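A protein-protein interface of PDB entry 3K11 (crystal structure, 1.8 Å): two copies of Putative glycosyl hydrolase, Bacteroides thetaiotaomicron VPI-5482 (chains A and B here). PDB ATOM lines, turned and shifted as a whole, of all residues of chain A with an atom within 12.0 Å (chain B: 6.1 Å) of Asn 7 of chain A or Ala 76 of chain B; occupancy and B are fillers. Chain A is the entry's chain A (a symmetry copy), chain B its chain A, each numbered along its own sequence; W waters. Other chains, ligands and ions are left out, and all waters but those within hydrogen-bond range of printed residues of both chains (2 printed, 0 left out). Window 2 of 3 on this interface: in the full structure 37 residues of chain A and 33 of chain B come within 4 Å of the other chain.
The guanidinium group of Arg 78 of chain B is in salt-bridge range of the side-chain carboxylate of Asp 8 of chain A (2.7 Å). The side-chain hydroxyl (OG) of Ser 9 of chain A sits close to the backbone carbonyl oxygen (O) of Gly 75 of chain B (2.4 Å). O of Ala 76 of chain B lies close to N of Asp 8 of chain A, at 3.0 Å. O of Ala 76 of chain B sits at hydrogen-bond distance from N of Ser 9 of chain A, 3.2 Å away.
N of Ser 9 of chain A sits at hydrogen-bond distance from OD1 of Asn 7 of chain A (3.2 Å). OD1 of Asn 393 of chain B sits at hydrogen-bond distance from N of Tyr 395 of chain B (2.8 Å). The backbone carbonyl oxygen (O) of Glu 46 of chain B lies within hydrogen-bond range of the backbone NH (N) of Phe 77 of chain B, 3.3 Å away. The backbone NH (N) of Asn 7 of chain A lies within hydrogen-bond range of the side-chain amide oxygen (OD1) of Asn 10 of chain A, 3.0 Å away. OE1 of Glu 46 of chain B sits at hydrogen-bond distance from N of Ala 76 of chain B, at 2.9 Å.
Among the printed residues, merely in contact across the chains: Ile 6 of chain A with Tyr 395 of chain B (3.4 Å), Asn 7 of chain A with Ala 76 of chain B (3.7 Å), Asn 7 of chain A with Tyr 395 of chain B (3.6 Å), Asp 8 of chain A with Phe 77 of chain B (3.6 Å), Asp 8 of chain A with Tyr 395 of chain B (3.3 Å), Ser 9 of chain A with Phe 77 of chain B (3.5 Å), Ser 9 of chain A with Arg 78 of chain B (3.8 Å) and Leu 13 of chain A with Tyr 395 of chain B (3.2 Å).
Of chain B, only Ala 76 and Tyr 395 come within 4 Å of Asn 7 of chain A. No residue of chain A comes within 4 Å of Glu 46 of chain B. No residue of chain A comes within 4 Å of Thr 47 of chain B. Of chain A, only Asp 8 (3.6 Å) and Ser 9 (3.5 Å) come within 4 Å of Phe 77 of chain B. Of chain A, only Ile 6, Asn 7, Asp 8 and Leu 13 come within 4 Å of Tyr 395 of chain B. Printed residues of chain B within 4 Å of Ser 9 of chain A: Gly 75 (2.4 Å), Ala 76 (3.2 Å), Phe 77 (3.5 Å) and Arg 78 (3.8 Å). Of the printed residues of chain B, Asp 8 of chain A touches Ala 76, Phe 77, Arg 78 and Tyr 395. Printed residues of chain B within 4 Å of Leu 13 of chain A: Tyr 395. Of the printed residues of chain A, Arg 78 of chain B touches Asp 8 (2.7 Å) and Ser 9 (3.8 Å). Of the printed residues of chain B, Ile 6 of chain A touches Tyr 395. Asn 393 of chain B touches none of the printed residues of chain A. Leu 16 of chain A touches none of the printed residues of chain B. The nearest printed residue of chain A that does not touch Arg 78 of chain B is Thr 11 of chain A (6.1 Å).
Along chain A the printed residues that touch a printed residue of chain B span positions 6 to 13. Hydrophobic or aromatic side chains of chain B that line the printed part of chain A: Phe 77 and Tyr 395. Along chain B the printed residues that touch a printed residue of chain A span positions 75 to 395. Among the printed residues, 12 pairs touch across the chains.
No position is printed for both chains. Of the 12 pairs that touch across the chains among the printed residues, none has its exchanged pair printed and touching as well.
Water W2 bridges OD2 of Asp 8 of chain A and O of Arg 78 of chain B. Water W1 lies within hydrogen-bond range of the side-chain amide nitrogen of Asn 7 of chain A (3.1 Å) and the side-chain hydroxyl of Tyr 395 of chain B (3.3 Å).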
ATOM      1  N   ILE A   6       5.922  16.900 -33.038  1.00  0.00           N
ATOM      2  CA  ILE A   6       6.144  16.907 -31.549  1.00  0.00           C
ATOM      3  C   ILE A   6       4.983  17.624 -30.831  1.00  0.00           C
ATOM      4  O   ILE A   6       4.956  18.855 -30.761  1.00  0.00           O
ATOM      5  CB  ILE A   6       7.514  17.579 -31.101  1.00  0.00           C
ATOM      6  CG1 ILE A   6       8.749  16.882 -31.731  1.00  0.00           C
ATOM      7  CG2 ILE A   6       7.626  17.624 -29.535  1.00  0.00           C
ATOM      8  CD1 ILE A   6       9.041  15.424 -31.240  1.00  0.00           C
ATOM      9  N   ASN A   7       4.038  16.847 -30.302  1.00  0.00           N
ATOM     10  CA  ASN A   7       2.894  17.390 -29.565  1.00  0.00           C
ATOM     11  C   ASN A   7       2.488  16.455 -28.399  1.00  0.00           C
ATOM     12  O   ASN A   7       3.223  15.499 -28.094  1.00  0.00           O
ATOM     13  CB  ASN A   7       1.745  17.694 -30.539  1.00  0.00           C
ATOM     14  CG  ASN A   7       1.256  16.463 -31.275  1.00  0.00           C
ATOM     15  OD1 ASN A   7       1.344  15.334 -30.766  1.00  0.00           O
ATOM     16  ND2 ASN A   7       0.713  16.676 -32.479  1.00  0.00           N
ATOM     17  N   ASP A   8       1.349  16.733 -27.743  1.00  0.00           N
ATOM     18  CA  ASP A   8       0.904  15.952 -26.547  1.00  0.00           C
ATOM     19  C   ASP A   8       0.614  14.440 -26.880  1.00  0.00           C
ATOM     20  O   ASP A   8       0.883  13.537 -26.070  1.00  0.00           O
ATOM     21  CB  ASP A   8      -0.307  16.634 -25.818  1.00  0.00           C
ATOM     22  CG  ASP A   8      -0.805  15.805 -24.612  1.00  0.00           C
ATOM     23  OD1 ASP A   8       0.080  15.620 -23.719  1.00  0.00           O
ATOM     24  OD2 ASP A   8      -2.016  15.329 -24.543  1.00  0.00           O
ATOM     25  N   SER A   9       0.097  14.176 -28.077  1.00  0.00           N
ATOM     26  CA  SER A   9      -0.226  12.809 -28.483  1.00  0.00           C
ATOM     27  C   SER A   9       0.986  11.963 -28.887  1.00  0.00           C
ATOM     28  O   SER A   9       0.993  10.747 -28.646  1.00  0.00           O
ATOM     29  CB  SER A   9      -1.190  12.839 -29.650  1.00  0.00           C
ATOM     30  OG  SER A   9      -2.408  13.443 -29.267  1.00  0.00           O
ATOM     31  N   ASN A  10       1.988  12.589 -29.519  1.00  0.00           N
ATOM     32  CA  ASN A  10       3.136  11.832 -30.055  1.00  0.00           C
ATOM     33  C   ASN A  10       4.479  12.037 -29.338  1.00  0.00           C
ATOM     34  O   ASN A  10       5.463  11.377 -29.698  1.00  0.00           O
ATOM     35  CB  ASN A  10       3.256  11.984 -31.604  1.00  0.00           C
ATOM     36  CG  ASN A  10       3.665  13.395 -32.072  1.00  0.00           C
ATOM     37  OD1 ASN A  10       4.412  14.115 -31.392  1.00  0.00           O
ATOM     38  ND2 ASN A  10       3.194  13.772 -33.273  1.00  0.00           N
ATOM     39  N   THR A  11       4.509  12.904 -28.318  1.00  0.00           N
ATOM     40  CA  THR A  11       5.742  13.159 -27.553  1.00  0.00           C
ATOM     41  C   THR A  11       5.512  13.189 -26.028  1.00  0.00           C
ATOM     42  O   THR A  11       4.480  13.730 -25.564  1.00  0.00           O
ATOM     43  CB  THR A  11       6.456  14.502 -28.004  1.00  0.00           C
ATOM     44  OG1 THR A  11       6.764  14.417 -29.400  1.00  0.00           O
ATOM     45  CG2 THR A  11       7.782  14.786 -27.204  1.00  0.00           C
ATOM     46  N   PRO A  12       6.476  12.589 -25.259  1.00  0.00           N
ATOM     47  CA  PRO A  12       6.571  12.817 -23.809  1.00  0.00           C
ATOM     48  C   PRO A  12       7.267  14.174 -23.610  1.00  0.00           C
ATOM     49  O   PRO A  12       8.513  14.267 -23.514  1.00  0.00           O
ATOM     50  CB  PRO A  12       7.426  11.649 -23.313  1.00  0.00           C
ATOM     51  CG  PRO A  12       8.322  11.317 -24.481  1.00  0.00           C
ATOM     52  CD  PRO A  12       7.536  11.663 -25.730  1.00  0.00           C
ATOM     53  N   LEU A  13       6.444  15.220 -23.626  1.00  0.00           N
ATOM     54  CA  LEU A  13       6.901  16.603 -23.409  1.00  0.00           C
ATOM     55  C   LEU A  13       7.574  16.693 -22.028  1.00  0.00           C
ATOM     56  O   LEU A  13       8.515  17.475 -21.836  1.00  0.00           O
ATOM     57  CB  LEU A  13       5.711  17.591 -23.526  1.00  0.00           C
ATOM     58  CG  LEU A  13       5.028  17.707 -24.898  1.00  0.00           C
ATOM     59  CD1 LEU A  13       3.710  18.471 -24.802  1.00  0.00           C
ATOM     60  CD2 LEU A  13       5.979  18.334 -25.899  1.00  0.00           C
ATOM     61  N   HIS A  14       7.081  15.877 -21.084  1.00  0.00           N
ATOM     62  CA  HIS A  14       7.642  15.777 -19.716  1.00  0.00           C
ATOM     63  C   HIS A  14       9.078  15.208 -19.619  1.00  0.00           C
ATOM     64  O   HIS A  14       9.710  15.272 -18.549  1.00  0.00           O
ATOM     65  CB  HIS A  14       6.731  14.932 -18.833  1.00  0.00           C
ATOM     66  CG  HIS A  14       6.634  13.490 -19.236  1.00  0.00           C
ATOM     67  ND1 HIS A  14       7.343  12.494 -18.600  1.00  0.00           N
ATOM     68  CD2 HIS A  14       5.889  12.873 -20.188  1.00  0.00           C
ATOM     69  CE1 HIS A  14       7.049  11.327 -19.150  1.00  0.00           C
ATOM     70  NE2 HIS A  14       6.168  11.529 -20.115  1.00  0.00           N
ATOM     71  N   LEU A  15       9.567  14.624 -20.714  1.00  0.00           N
ATOM     72  CA  LEU A  15      10.925  14.112 -20.780  1.00  0.00           C
ATOM     73  C   LEU A  15      11.846  15.008 -21.638  1.00  0.00           C
ATOM     74  O   LEU A  15      13.008  14.662 -21.795  1.00  0.00           O
ATOM     75  CB  LEU A  15      10.925  12.621 -21.226  1.00  0.00           C
ATOM     76  CG  LEU A  15      10.561  11.588 -20.111  1.00  0.00           C
ATOM     77  CD1 LEU A  15      10.119  10.242 -20.697  1.00  0.00           C
ATOM     78  CD2 LEU A  15      11.675  11.344 -19.012  1.00  0.00           C
ATOM     79  N   LEU A  16      11.352  16.156 -22.143  1.00  0.00           N
ATOM     80  CA  LEU A  16      12.189  17.148 -22.903  1.00  0.00           C
ATOM     81  C   LEU A  16      13.367  17.654 -22.082  1.00  0.00           C
ATOM     82  O   LEU A  16      13.215  17.891 -20.865  1.00  0.00           O
ATOM     83  CB  LEU A  16      11.407  18.417 -23.307  1.00  0.00           C
ATOM     84  CG  LEU A  16      10.384  18.414 -24.434  1.00  0.00           C
ATOM     85  CD1 LEU A  16       9.636  19.780 -24.531  1.00  0.00           C
ATOM     86  CD2 LEU A  16      11.095  18.063 -25.723  1.00  0.00           C
ATOM     87  N   TYR B  42      -9.898  25.670 -31.479  1.00  0.00           N
ATOM     88  CA  TYR B  42      -8.629  25.014 -31.689  1.00  0.00           C
ATOM     89  C   TYR B  42      -8.603  23.587 -31.152  1.00  0.00           C
ATOM     90  O   TYR B  42      -8.241  22.671 -31.853  1.00  0.00           O
ATOM     91  CB  TYR B  42      -7.517  25.844 -31.040  1.00  0.00           C
ATOM     92  CG  TYR B  42      -6.171  25.163 -31.108  1.00  0.00           C
ATOM     93  CD1 TYR B  42      -5.549  24.931 -32.317  1.00  0.00           C
ATOM     94  CD2 TYR B  42      -5.519  24.776 -29.965  1.00  0.00           C
ATOM     95  CE1 TYR B  42      -4.318  24.288 -32.369  1.00  0.00           C
ATOM     96  CE2 TYR B  42      -4.302  24.136 -30.015  1.00  0.00           C
ATOM     97  CZ  TYR B  42      -3.701  23.905 -31.206  1.00  0.00           C
ATOM     98  OH  TYR B  42      -2.470  23.258 -31.198  1.00  0.00           O
ATOM     99  N   GLU B  46      -8.208  19.501 -32.791  1.00  0.00           N
ATOM    100  CA  GLU B  46      -7.044  18.742 -32.342  1.00  0.00           C
ATOM    101  C   GLU B  46      -7.314  17.574 -31.427  1.00  0.00           C
ATOM    102  O   GLU B  46      -6.376  17.010 -30.826  1.00  0.00           O
ATOM    103  CB  GLU B  46      -6.093  19.714 -31.634  1.00  0.00           C
ATOM    104  CG  GLU B  46      -5.434  20.682 -32.585  1.00  0.00           C
ATOM    105  CD  GLU B  46      -4.509  19.974 -33.575  1.00  0.00           C
ATOM    106  OE1 GLU B  46      -4.212  18.765 -33.418  1.00  0.00           O
ATOM    107  OE2 GLU B  46      -4.090  20.635 -34.509  1.00  0.00           O
ATOM    108  N   THR B  47      -8.587  17.246 -31.240  1.00  0.00           N
ATOM    109  CA  THR B  47      -8.988  16.118 -30.419  1.00  0.00           C
ATOM    110  C   THR B  47     -10.004  15.261 -31.173  1.00  0.00           C
ATOM    111  O   THR B  47     -11.121  15.043 -30.695  1.00  0.00           O
ATOM    112  CB  THR B  47      -9.530  16.594 -29.056  1.00  0.00           C
ATOM    113  OG1 THR B  47     -10.558  17.593 -29.229  1.00  0.00           O
ATOM    114  CG2 THR B  47      -8.352  17.151 -28.187  1.00  0.00           C
ATOM    115  N   PRO B  48      -9.590  14.694 -32.313  1.00  0.00           N
ATOM    116  CA  PRO B  48     -10.521  13.926 -33.143  1.00  0.00           C
ATOM    117  C   PRO B  48     -11.074  12.692 -32.433  1.00  0.00           C
ATOM    118  O   PRO B  48     -10.352  11.983 -31.790  1.00  0.00           O
ATOM    119  CB  PRO B  48      -9.678  13.532 -34.355  1.00  0.00           C
ATOM    120  CG  PRO B  48      -8.251  13.547 -33.878  1.00  0.00           C
ATOM    121  CD  PRO B  48      -8.229  14.700 -32.897  1.00  0.00           C
ATOM    122  N   ARG B  74      -4.531  10.423 -33.759  1.00  0.00           N
ATOM    123  CA  ARG B  74      -3.723  11.263 -32.919  1.00  0.00           C
ATOM    124  C   ARG B  74      -3.850  12.720 -33.330  1.00  0.00           C
ATOM    125  O   ARG B  74      -3.389  13.102 -34.391  1.00  0.00           O
ATOM    126  CB  ARG B  74      -2.271  10.830 -33.010  1.00  0.00           C
ATOM    127  CG  ARG B  74      -2.004   9.372 -32.697  1.00  0.00           C
ATOM    128  CD  ARG B  74      -2.380   9.066 -31.348  1.00  0.00           C
ATOM    129  NE  ARG B  74      -1.788   7.838 -30.804  1.00  0.00           N
ATOM    130  CZ  ARG B  74      -2.456   6.804 -30.290  1.00  0.00           C
ATOM    131  NH1 ARG B  74      -3.778   6.695 -30.384  1.00  0.00           N
ATOM    132  NH2 ARG B  74      -1.783   5.843 -29.694  1.00  0.00           N
ATOM    133  N   GLY B  75      -4.521  13.512 -32.526  1.00  0.00           N
ATOM    134  CA  GLY B  75      -4.522  14.974 -32.673  1.00  0.00           C
ATOM    135  C   GLY B  75      -3.452  15.496 -31.733  1.00  0.00           C
ATOM    136  O   GLY B  75      -2.661  14.717 -31.234  1.00  0.00           O
ATOM    137  N   ALA B  76      -3.413  16.796 -31.470  1.00  0.00           N
ATOM    138  CA  ALA B  76      -2.371  17.341 -30.591  1.00  0.00           C
ATOM    139  C   ALA B  76      -2.557  16.934 -29.159  1.00  0.00           C
ATOM    140  O   ALA B  76      -1.585  16.876 -28.426  1.00  0.00           O
ATOM    141  CB  ALA B  76      -2.300  18.904 -30.704  1.00  0.00           C
ATOM    142  N   PHE B  77      -3.794  16.636 -28.732  1.00  0.00           N
ATOM    143  CA  PHE B  77      -4.048  16.320 -27.336  1.00  0.00           C
ATOM    144  C   PHE B  77      -4.795  15.004 -27.167  1.00  0.00           C
ATOM    145  O   PHE B  77      -5.710  14.717 -27.950  1.00  0.00           O
ATOM    146  CB  PHE B  77      -4.889  17.420 -26.736  1.00  0.00           C
ATOM    147  CG  PHE B  77      -4.305  18.776 -26.948  1.00  0.00           C
ATOM    148  CD1 PHE B  77      -3.125  19.127 -26.292  1.00  0.00           C
ATOM    149  CD2 PHE B  77      -4.860  19.652 -27.882  1.00  0.00           C
ATOM    150  CE1 PHE B  77      -2.531  20.348 -26.544  1.00  0.00           C
ATOM    151  CE2 PHE B  77      -4.290  20.880 -28.110  1.00  0.00           C
ATOM    152  CZ  PHE B  77      -3.107  21.227 -27.420  1.00  0.00           C
ATOM    153  N   ARG B  78      -4.412  14.233 -26.139  1.00  0.00           N
ATOM    154  CA  ARG B  78      -5.016  12.916 -25.842  1.00  0.00           C
ATOM    155  C   ARG B  78      -6.387  13.137 -25.230  1.00  0.00           C
ATOM    156  O   ARG B  78      -6.574  14.066 -24.435  1.00  0.00           O
ATOM    157  CB  ARG B  78      -4.109  12.116 -24.882  1.00  0.00           C
ATOM    158  CG  ARG B  78      -2.792  11.652 -25.490  1.00  0.00           C
ATOM    159  CD  ARG B  78      -1.688  11.265 -24.476  1.00  0.00           C
ATOM    160  NE  ARG B  78      -1.204  12.461 -23.756  1.00  0.00           N
ATOM    161  CZ  ARG B  78      -1.115  12.613 -22.424  1.00  0.00           C
ATOM    162  NH1 ARG B  78      -1.404  11.618 -21.572  1.00  0.00           N
ATOM    163  NH2 ARG B  78      -0.699  13.778 -21.936  1.00  0.00           N
ATOM    164  N   ASN B 393       5.673  24.625 -23.275  1.00  0.00           N
ATOM    165  CA  ASN B 393       5.355  24.271 -24.636  1.00  0.00           C
ATOM    166  C   ASN B 393       3.868  24.448 -24.881  1.00  0.00           C
ATOM    167  O   ASN B 393       3.073  24.141 -24.005  1.00  0.00           O
ATOM    168  CB  ASN B 393       5.747  22.821 -24.932  1.00  0.00           C
ATOM    169  CG  ASN B 393       5.790  22.546 -26.406  1.00  0.00           C
ATOM    170  OD1 ASN B 393       4.777  22.216 -26.994  1.00  0.00           O
ATOM    171  ND2 ASN B 393       6.935  22.818 -27.038  1.00  0.00           N
ATOM    172  N   TYR B 395       2.039  22.707 -26.618  1.00  0.00           N
ATOM    173  CA  TYR B 395       1.363  21.428 -26.572  1.00  0.00           C
ATOM    174  C   TYR B 395       1.243  20.771 -25.194  1.00  0.00           C
ATOM    175  O   TYR B 395       0.739  19.655 -25.098  1.00  0.00           O
ATOM    176  CB  TYR B 395       2.012  20.454 -27.542  1.00  0.00           C
ATOM    177  CG  TYR B 395       1.819  20.903 -28.968  1.00  0.00           C
ATOM    178  CD1 TYR B 395       0.543  20.949 -29.511  1.00  0.00           C
ATOM    179  CD2 TYR B 395       2.896  21.319 -29.753  1.00  0.00           C
ATOM    180  CE1 TYR B 395       0.325  21.374 -30.791  1.00  0.00           C
ATOM    181  CE2 TYR B 395       2.678  21.756 -31.062  1.00  0.00           C
ATOM    182  CZ  TYR B 395       1.380  21.775 -31.561  1.00  0.00           C
ATOM    183  OH  TYR B 395       1.095  22.167 -32.868  1.00  0.00           O
HETATM  184  O   HOH W   1      -0.055  19.288 -34.032  1.00  0.00           O
HETATM  185  O   HOH W   2      -4.315  15.600 -23.304  1.00  0.00           O
